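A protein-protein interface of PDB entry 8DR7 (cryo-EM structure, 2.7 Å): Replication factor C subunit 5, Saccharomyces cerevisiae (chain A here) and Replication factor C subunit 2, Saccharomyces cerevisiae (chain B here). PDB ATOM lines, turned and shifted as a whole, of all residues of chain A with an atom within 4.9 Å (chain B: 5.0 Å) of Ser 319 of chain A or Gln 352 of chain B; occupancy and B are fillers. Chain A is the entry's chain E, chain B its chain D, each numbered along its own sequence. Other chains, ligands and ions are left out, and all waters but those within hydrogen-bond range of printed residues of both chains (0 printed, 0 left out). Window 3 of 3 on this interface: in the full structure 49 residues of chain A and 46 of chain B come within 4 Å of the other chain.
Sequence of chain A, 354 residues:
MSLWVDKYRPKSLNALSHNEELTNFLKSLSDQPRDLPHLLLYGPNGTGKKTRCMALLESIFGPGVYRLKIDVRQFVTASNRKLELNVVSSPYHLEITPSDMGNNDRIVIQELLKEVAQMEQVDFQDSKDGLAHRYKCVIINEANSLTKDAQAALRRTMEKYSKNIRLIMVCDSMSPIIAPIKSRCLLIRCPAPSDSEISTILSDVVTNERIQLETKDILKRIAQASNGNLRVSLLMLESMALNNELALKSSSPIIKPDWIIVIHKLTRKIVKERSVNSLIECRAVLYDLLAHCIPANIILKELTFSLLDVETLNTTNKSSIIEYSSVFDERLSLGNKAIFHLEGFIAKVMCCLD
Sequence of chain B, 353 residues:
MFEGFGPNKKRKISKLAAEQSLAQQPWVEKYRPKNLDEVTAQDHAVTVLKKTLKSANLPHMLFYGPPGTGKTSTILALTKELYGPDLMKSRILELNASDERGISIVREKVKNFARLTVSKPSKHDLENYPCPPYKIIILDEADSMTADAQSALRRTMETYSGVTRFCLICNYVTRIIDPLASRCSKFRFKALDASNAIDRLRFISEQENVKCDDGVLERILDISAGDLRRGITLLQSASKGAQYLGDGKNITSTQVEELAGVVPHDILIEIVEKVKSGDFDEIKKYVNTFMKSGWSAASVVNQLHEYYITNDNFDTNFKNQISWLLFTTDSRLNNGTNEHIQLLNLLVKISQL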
ATOM      1  N   THR A 315      12.391  32.213  31.668  1.00  0.00           N
ATOM      2  CA  THR A 315      11.017  31.814  31.378  1.00  0.00           C
ATOM      3  C   THR A 315      10.793  31.614  29.884  1.00  0.00           C
ATOM      4  O   THR A 315      10.131  30.654  29.473  1.00  0.00           O
ATOM      5  CB  THR A 315      10.044  32.859  31.926  1.00  0.00           C
ATOM      6  OG1 THR A 315      10.169  32.933  33.352  1.00  0.00           O
ATOM      7  CG2 THR A 315       8.608  32.501  31.563  1.00  0.00           C
ATOM      8  N   THR A 316      11.328  32.514  29.054  1.00  0.00           N
ATOM      9  CA  THR A 316      11.114  32.405  27.614  1.00  0.00           C
ATOM     10  C   THR A 316      11.726  31.123  27.061  1.00  0.00           C
ATOM     11  O   THR A 316      11.113  30.440  26.230  1.00  0.00           O
ATOM     12  CB  THR A 316      11.703  33.625  26.903  1.00  0.00           C
ATOM     13  OG1 THR A 316      11.210  34.823  27.517  1.00  0.00           O
ATOM     14  CG2 THR A 316      11.325  33.621  25.429  1.00  0.00           C
ATOM     15  N   ASN A 317      12.937  30.784  27.507  1.00  0.00           N
ATOM     16  CA  ASN A 317      13.578  29.560  27.040  1.00  0.00           C
ATOM     17  C   ASN A 317      12.769  28.334  27.440  1.00  0.00           C
ATOM     18  O   ASN A 317      12.592  27.409  26.639  1.00  0.00           O
ATOM     19  CB  ASN A 317      14.999  29.471  27.594  1.00  0.00           C
ATOM     20  CG  ASN A 317      15.938  30.473  26.953  1.00  0.00           C
ATOM     21  OD1 ASN A 317      15.588  31.131  25.974  1.00  0.00           O
ATOM     22  ND2 ASN A 317      17.140  30.595  27.505  1.00  0.00           N
ATOM     23  N   LYS A 318      12.269  28.308  28.677  1.00  0.00           N
ATOM     24  CA  LYS A 318      11.466  27.177  29.127  1.00  0.00           C
ATOM     25  C   LYS A 318      10.171  27.070  28.331  1.00  0.00           C
ATOM     26  O   LYS A 318       9.738  25.965  27.979  1.00  0.00           O
ATOM     27  CB  LYS A 318      11.172  27.310  30.620  1.00  0.00           C
ATOM     28  CG  LYS A 318      12.361  26.988  31.512  1.00  0.00           C
ATOM     29  CD  LYS A 318      12.120  27.432  32.945  1.00  0.00           C
ATOM     30  CE  LYS A 318      13.280  27.047  33.849  1.00  0.00           C
ATOM     31  NZ  LYS A 318      13.723  28.180  34.706  1.00  0.00           N
ATOM     32  N   SER A 319       9.530  28.207  28.047  1.00  0.00           N
ATOM     33  CA  SER A 319       8.306  28.183  27.254  1.00  0.00           C
ATOM     34  C   SER A 319       8.572  27.655  25.851  1.00  0.00           C
ATOM     35  O   SER A 319       7.805  26.834  25.328  1.00  0.00           O
ATOM     36  CB  SER A 319       7.700  29.585  27.191  1.00  0.00           C
ATOM     37  OG  SER A 319       7.406  30.072  28.489  1.00  0.00           O
ATOM     38  N   SER A 320       9.660  28.105  25.224  1.00  0.00           N
ATOM     39  CA  SER A 320      10.005  27.597  23.901  1.00  0.00           C
ATOM     40  C   SER A 320      10.289  26.101  23.951  1.00  0.00           C
ATOM     41  O   SER A 320       9.862  25.348  23.066  1.00  0.00           O
ATOM     42  CB  SER A 320      11.211  28.354  23.347  1.00  0.00           C
ATOM     43  OG  SER A 320      10.897  29.718  23.124  1.00  0.00           O
ATOM     44  N   ILE A 321      11.002  25.653  24.986  1.00  0.00           N
ATOM     45  CA  ILE A 321      11.339  24.238  25.105  1.00  0.00           C
ATOM     46  C   ILE A 321      10.077  23.400  25.248  1.00  0.00           C
ATOM     47  O   ILE A 321       9.935  22.353  24.606  1.00  0.00           O
ATOM     48  CB  ILE A 321      12.301  24.020  26.288  1.00  0.00           C
ATOM     49  CG1 ILE A 321      13.709  24.487  25.918  1.00  0.00           C
ATOM     50  CG2 ILE A 321      12.323  22.553  26.698  1.00  0.00           C
ATOM     51  CD1 ILE A 321      14.584  24.793  27.115  1.00  0.00           C
ATOM     52  N   ILE A 322       9.139  23.839  26.092  1.00  0.00           N
ATOM     53  CA  ILE A 322       7.926  23.056  26.303  1.00  0.00           C
ATOM     54  C   ILE A 322       7.056  23.064  25.051  1.00  0.00           C
ATOM     55  O   ILE A 322       6.429  22.053  24.715  1.00  0.00           O
ATOM     56  CB  ILE A 322       7.161  23.556  27.546  1.00  0.00           C
ATOM     57  CG1 ILE A 322       6.113  22.527  27.983  1.00  0.00           C
ATOM     58  CG2 ILE A 322       6.499  24.899  27.290  1.00  0.00           C
ATOM     59  CD1 ILE A 322       6.685  21.186  28.400  1.00  0.00           C
ATOM     60  N   GLU A 323       7.000  24.192  24.337  1.00  0.00           N
ATOM     61  CA  GLU A 323       6.245  24.216  23.086  1.00  0.00           C
ATOM     62  C   GLU A 323       6.839  23.251  22.065  1.00  0.00           C
ATOM     63  O   GLU A 323       6.106  22.497  21.407  1.00  0.00           O
ATOM     64  CB  GLU A 323       6.213  25.637  22.523  1.00  0.00           C
ATOM     65  CG  GLU A 323       4.926  25.978  21.785  1.00  0.00           C
ATOM     66  CD  GLU A 323       5.158  26.865  20.575  1.00  0.00           C
ATOM     67  OE1 GLU A 323       4.254  26.945  19.716  1.00  0.00           O
ATOM     68  OE2 GLU A 323       6.238  27.486  20.482  1.00  0.00           O
ATOM     69  N   PHE B 280       6.369  30.277  36.087  1.00  0.00           N
ATOM     70  CA  PHE B 280       6.548  29.006  35.392  1.00  0.00           C
ATOM     71  C   PHE B 280       6.855  27.876  36.366  1.00  0.00           C
ATOM     72  O   PHE B 280       6.301  26.777  36.243  1.00  0.00           O
ATOM     73  CB  PHE B 280       7.664  29.131  34.354  1.00  0.00           C
ATOM     74  CG  PHE B 280       7.795  27.933  33.458  1.00  0.00           C
ATOM     75  CD1 PHE B 280       8.582  26.855  33.828  1.00  0.00           C
ATOM     76  CD2 PHE B 280       7.132  27.883  32.243  1.00  0.00           C
ATOM     77  CE1 PHE B 280       8.704  25.752  33.007  1.00  0.00           C
ATOM     78  CE2 PHE B 280       7.251  26.781  31.417  1.00  0.00           C
ATOM     79  CZ  PHE B 280       8.036  25.715  31.799  1.00  0.00           C
ATOM     80  N   ASN B 345       2.007  22.690  28.689  1.00  0.00           N
ATOM     81  CA  ASN B 345       2.105  23.690  27.633  1.00  0.00           C
ATOM     82  C   ASN B 345       0.848  24.549  27.569  1.00  0.00           C
ATOM     83  O   ASN B 345       0.931  25.774  27.430  1.00  0.00           O
ATOM     84  CB  ASN B 345       2.356  23.009  26.288  1.00  0.00           C
ATOM     85  CG  ASN B 345       2.592  24.000  25.167  1.00  0.00           C
ATOM     86  OD1 ASN B 345       3.233  25.033  25.360  1.00  0.00           O
ATOM     87  ND2 ASN B 345       2.074  23.690  23.984  1.00  0.00           N
ATOM     88  N   VAL B 348       0.811  26.940  30.555  1.00  0.00           N
ATOM     89  CA  VAL B 348       1.807  27.994  30.381  1.00  0.00           C
ATOM     90  C   VAL B 348       1.322  29.020  29.367  1.00  0.00           C
ATOM     91  O   VAL B 348       1.456  30.233  29.574  1.00  0.00           O
ATOM     92  CB  VAL B 348       3.160  27.384  29.970  1.00  0.00           C
ATOM     93  CG1 VAL B 348       4.090  28.460  29.423  1.00  0.00           C
ATOM     94  CG2 VAL B 348       3.799  26.669  31.149  1.00  0.00           C
ATOM     95  N   LYS B 349       0.754  28.554  28.252  1.00  0.00           N
ATOM     96  CA  LYS B 349       0.256  29.478  27.239  1.00  0.00           C
ATOM     97  C   LYS B 349      -0.879  30.336  27.783  1.00  0.00           C
ATOM     98  O   LYS B 349      -0.938  31.542  27.515  1.00  0.00           O
ATOM     99  CB  LYS B 349      -0.203  28.704  26.004  1.00  0.00           C
ATOM    100  CG  LYS B 349       0.938  28.114  25.188  1.00  0.00           C
ATOM    101  CD  LYS B 349       0.675  28.196  23.691  1.00  0.00           C
ATOM    102  CE  LYS B 349       1.974  28.266  22.908  1.00  0.00           C
ATOM    103  NZ  LYS B 349       1.749  28.200  21.438  1.00  0.00           N
ATOM    104  N   ILE B 350      -1.790  29.734  28.550  1.00  0.00           N
ATOM    105  CA  ILE B 350      -2.889  30.505  29.123  1.00  0.00           C
ATOM    106  C   ILE B 350      -2.354  31.543  30.101  1.00  0.00           C
ATOM    107  O   ILE B 350      -2.825  32.687  30.133  1.00  0.00           O
ATOM    108  CB  ILE B 350      -3.912  29.570  29.794  1.00  0.00           C
ATOM    109  CG1 ILE B 350      -4.548  28.640  28.758  1.00  0.00           C
ATOM    110  CG2 ILE B 350      -5.001  30.380  30.487  1.00  0.00           C
ATOM    111  CD1 ILE B 350      -5.256  27.448  29.362  1.00  0.00           C
ATOM    112  N   SER B 351      -1.365  31.166  30.915  1.00  0.00           N
ATOM    113  CA  SER B 351      -0.815  32.095  31.895  1.00  0.00           C
ATOM    114  C   SER B 351      -0.176  33.314  31.243  1.00  0.00           C
ATOM    115  O   SER B 351      -0.099  34.371  31.878  1.00  0.00           O
ATOM    116  CB  SER B 351       0.213  31.379  32.772  1.00  0.00           C
ATOM    117  OG  SER B 351       1.461  31.273  32.110  1.00  0.00           O
ATOM    118  N   GLN B 352       0.281  33.195  29.999  1.00  0.00           N
ATOM    119  CA  GLN B 352       0.922  34.294  29.290  1.00  0.00           C
ATOM    120  C   GLN B 352      -0.052  35.087  28.428  1.00  0.00           C
ATOM    121  O   GLN B 352       0.369  36.016  27.732  1.00  0.00           O
ATOM    122  CB  GLN B 352       2.068  33.763  28.426  1.00  0.00           C
ATOM    123  CG  GLN B 352       3.222  33.177  29.223  1.00  0.00           C
ATOM    124  CD  GLN B 352       4.246  32.486  28.346  1.00  0.00           C
ATOM    125  OE1 GLN B 352       4.107  32.445  27.124  1.00  0.00           O
ATOM    126  NE2 GLN B 352       5.284  31.939  28.966  1.00  0.00           N
ATOM    127  N   LEU B 353      -1.336  34.745  28.455  1.00  0.00           N
ATOM    128  CA  LEU B 353      -2.335  35.470  27.677  1.00  0.00           C
ATOM    129  C   LEU B 353      -2.605  36.836  28.297  1.00  0.00           C
ATOM    130  O   LEU B 353      -3.141  37.733  27.646  1.00  0.00           O
ATOM    131  CB  LEU B 353      -3.637  34.668  27.588  1.00  0.00           C
ATOM    132  CG  LEU B 353      -3.702  33.508  26.589  1.00  0.00           C
ATOM    133  CD1 LEU B 353      -5.134  33.013  26.460  1.00  0.00           C
ATOM    134  CD2 LEU B 353      -3.152  33.899  25.224  1.00  0.00           C
ATOM    135  OXT LEU B 353      -2.293  37.076  29.464  1.00  0.00           O
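The side-chain hydroxyl (OG) of Ser 319 of chain A sits at hydrogen-bond distance from the side-chain amide nitrogen (NE2) of Gln 352 of chain B, 2.9 Å away.
The side-chain carboxylate of Glu 323 of chain A lies within salt-bridge range of the side-chain amino group of Lys 349 of chain B, at 3.3 Å.
O of Val 348 of chain B lies within hydrogen-bond range of OG of Ser 351 of chain B (2.7 Å).
OG of Ser 319 of chain A lies within hydrogen-bond range of O of Thr 315 of chain A (3.0 Å).
Among the printed residues, pairs that only touch across the chains: Lys 318 of chain A with Phe 280 of chain B, Ile 322 of chain A with Asn 345 of chain B, Ser 319 of chain A with Val 348 of chain B and Glu 323 of chain A with Asn 345 of chain B.
Of chain B, only Val 348 (3.8 Å) and Gln 352 (2.9 Å) come within 4 Å of Ser 319 of chain A.
Of chain A, only Ser 319 comes within 4 Å of Gln 352 of chain B.
Printed residues of chain B within 4 Å of Ile 322 of chain A: Asn 345 (3.8 Å).
Of the printed residues of chain A, Lys 349 of chain B touches Glu 323 (3.3 Å).
The nearest residue of chain A that does not touch Gln 352 of chain B is Thr 315 of chain A (4.3 Å).
Hydrophobic or aromatic side chains of chain A that line the printed part of chain B: Ile 322.
Printed residues of chain B that touch a printed residue of chain A: Phe 280, Asn 345, Val 348, Lys 349 and Gln 352.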
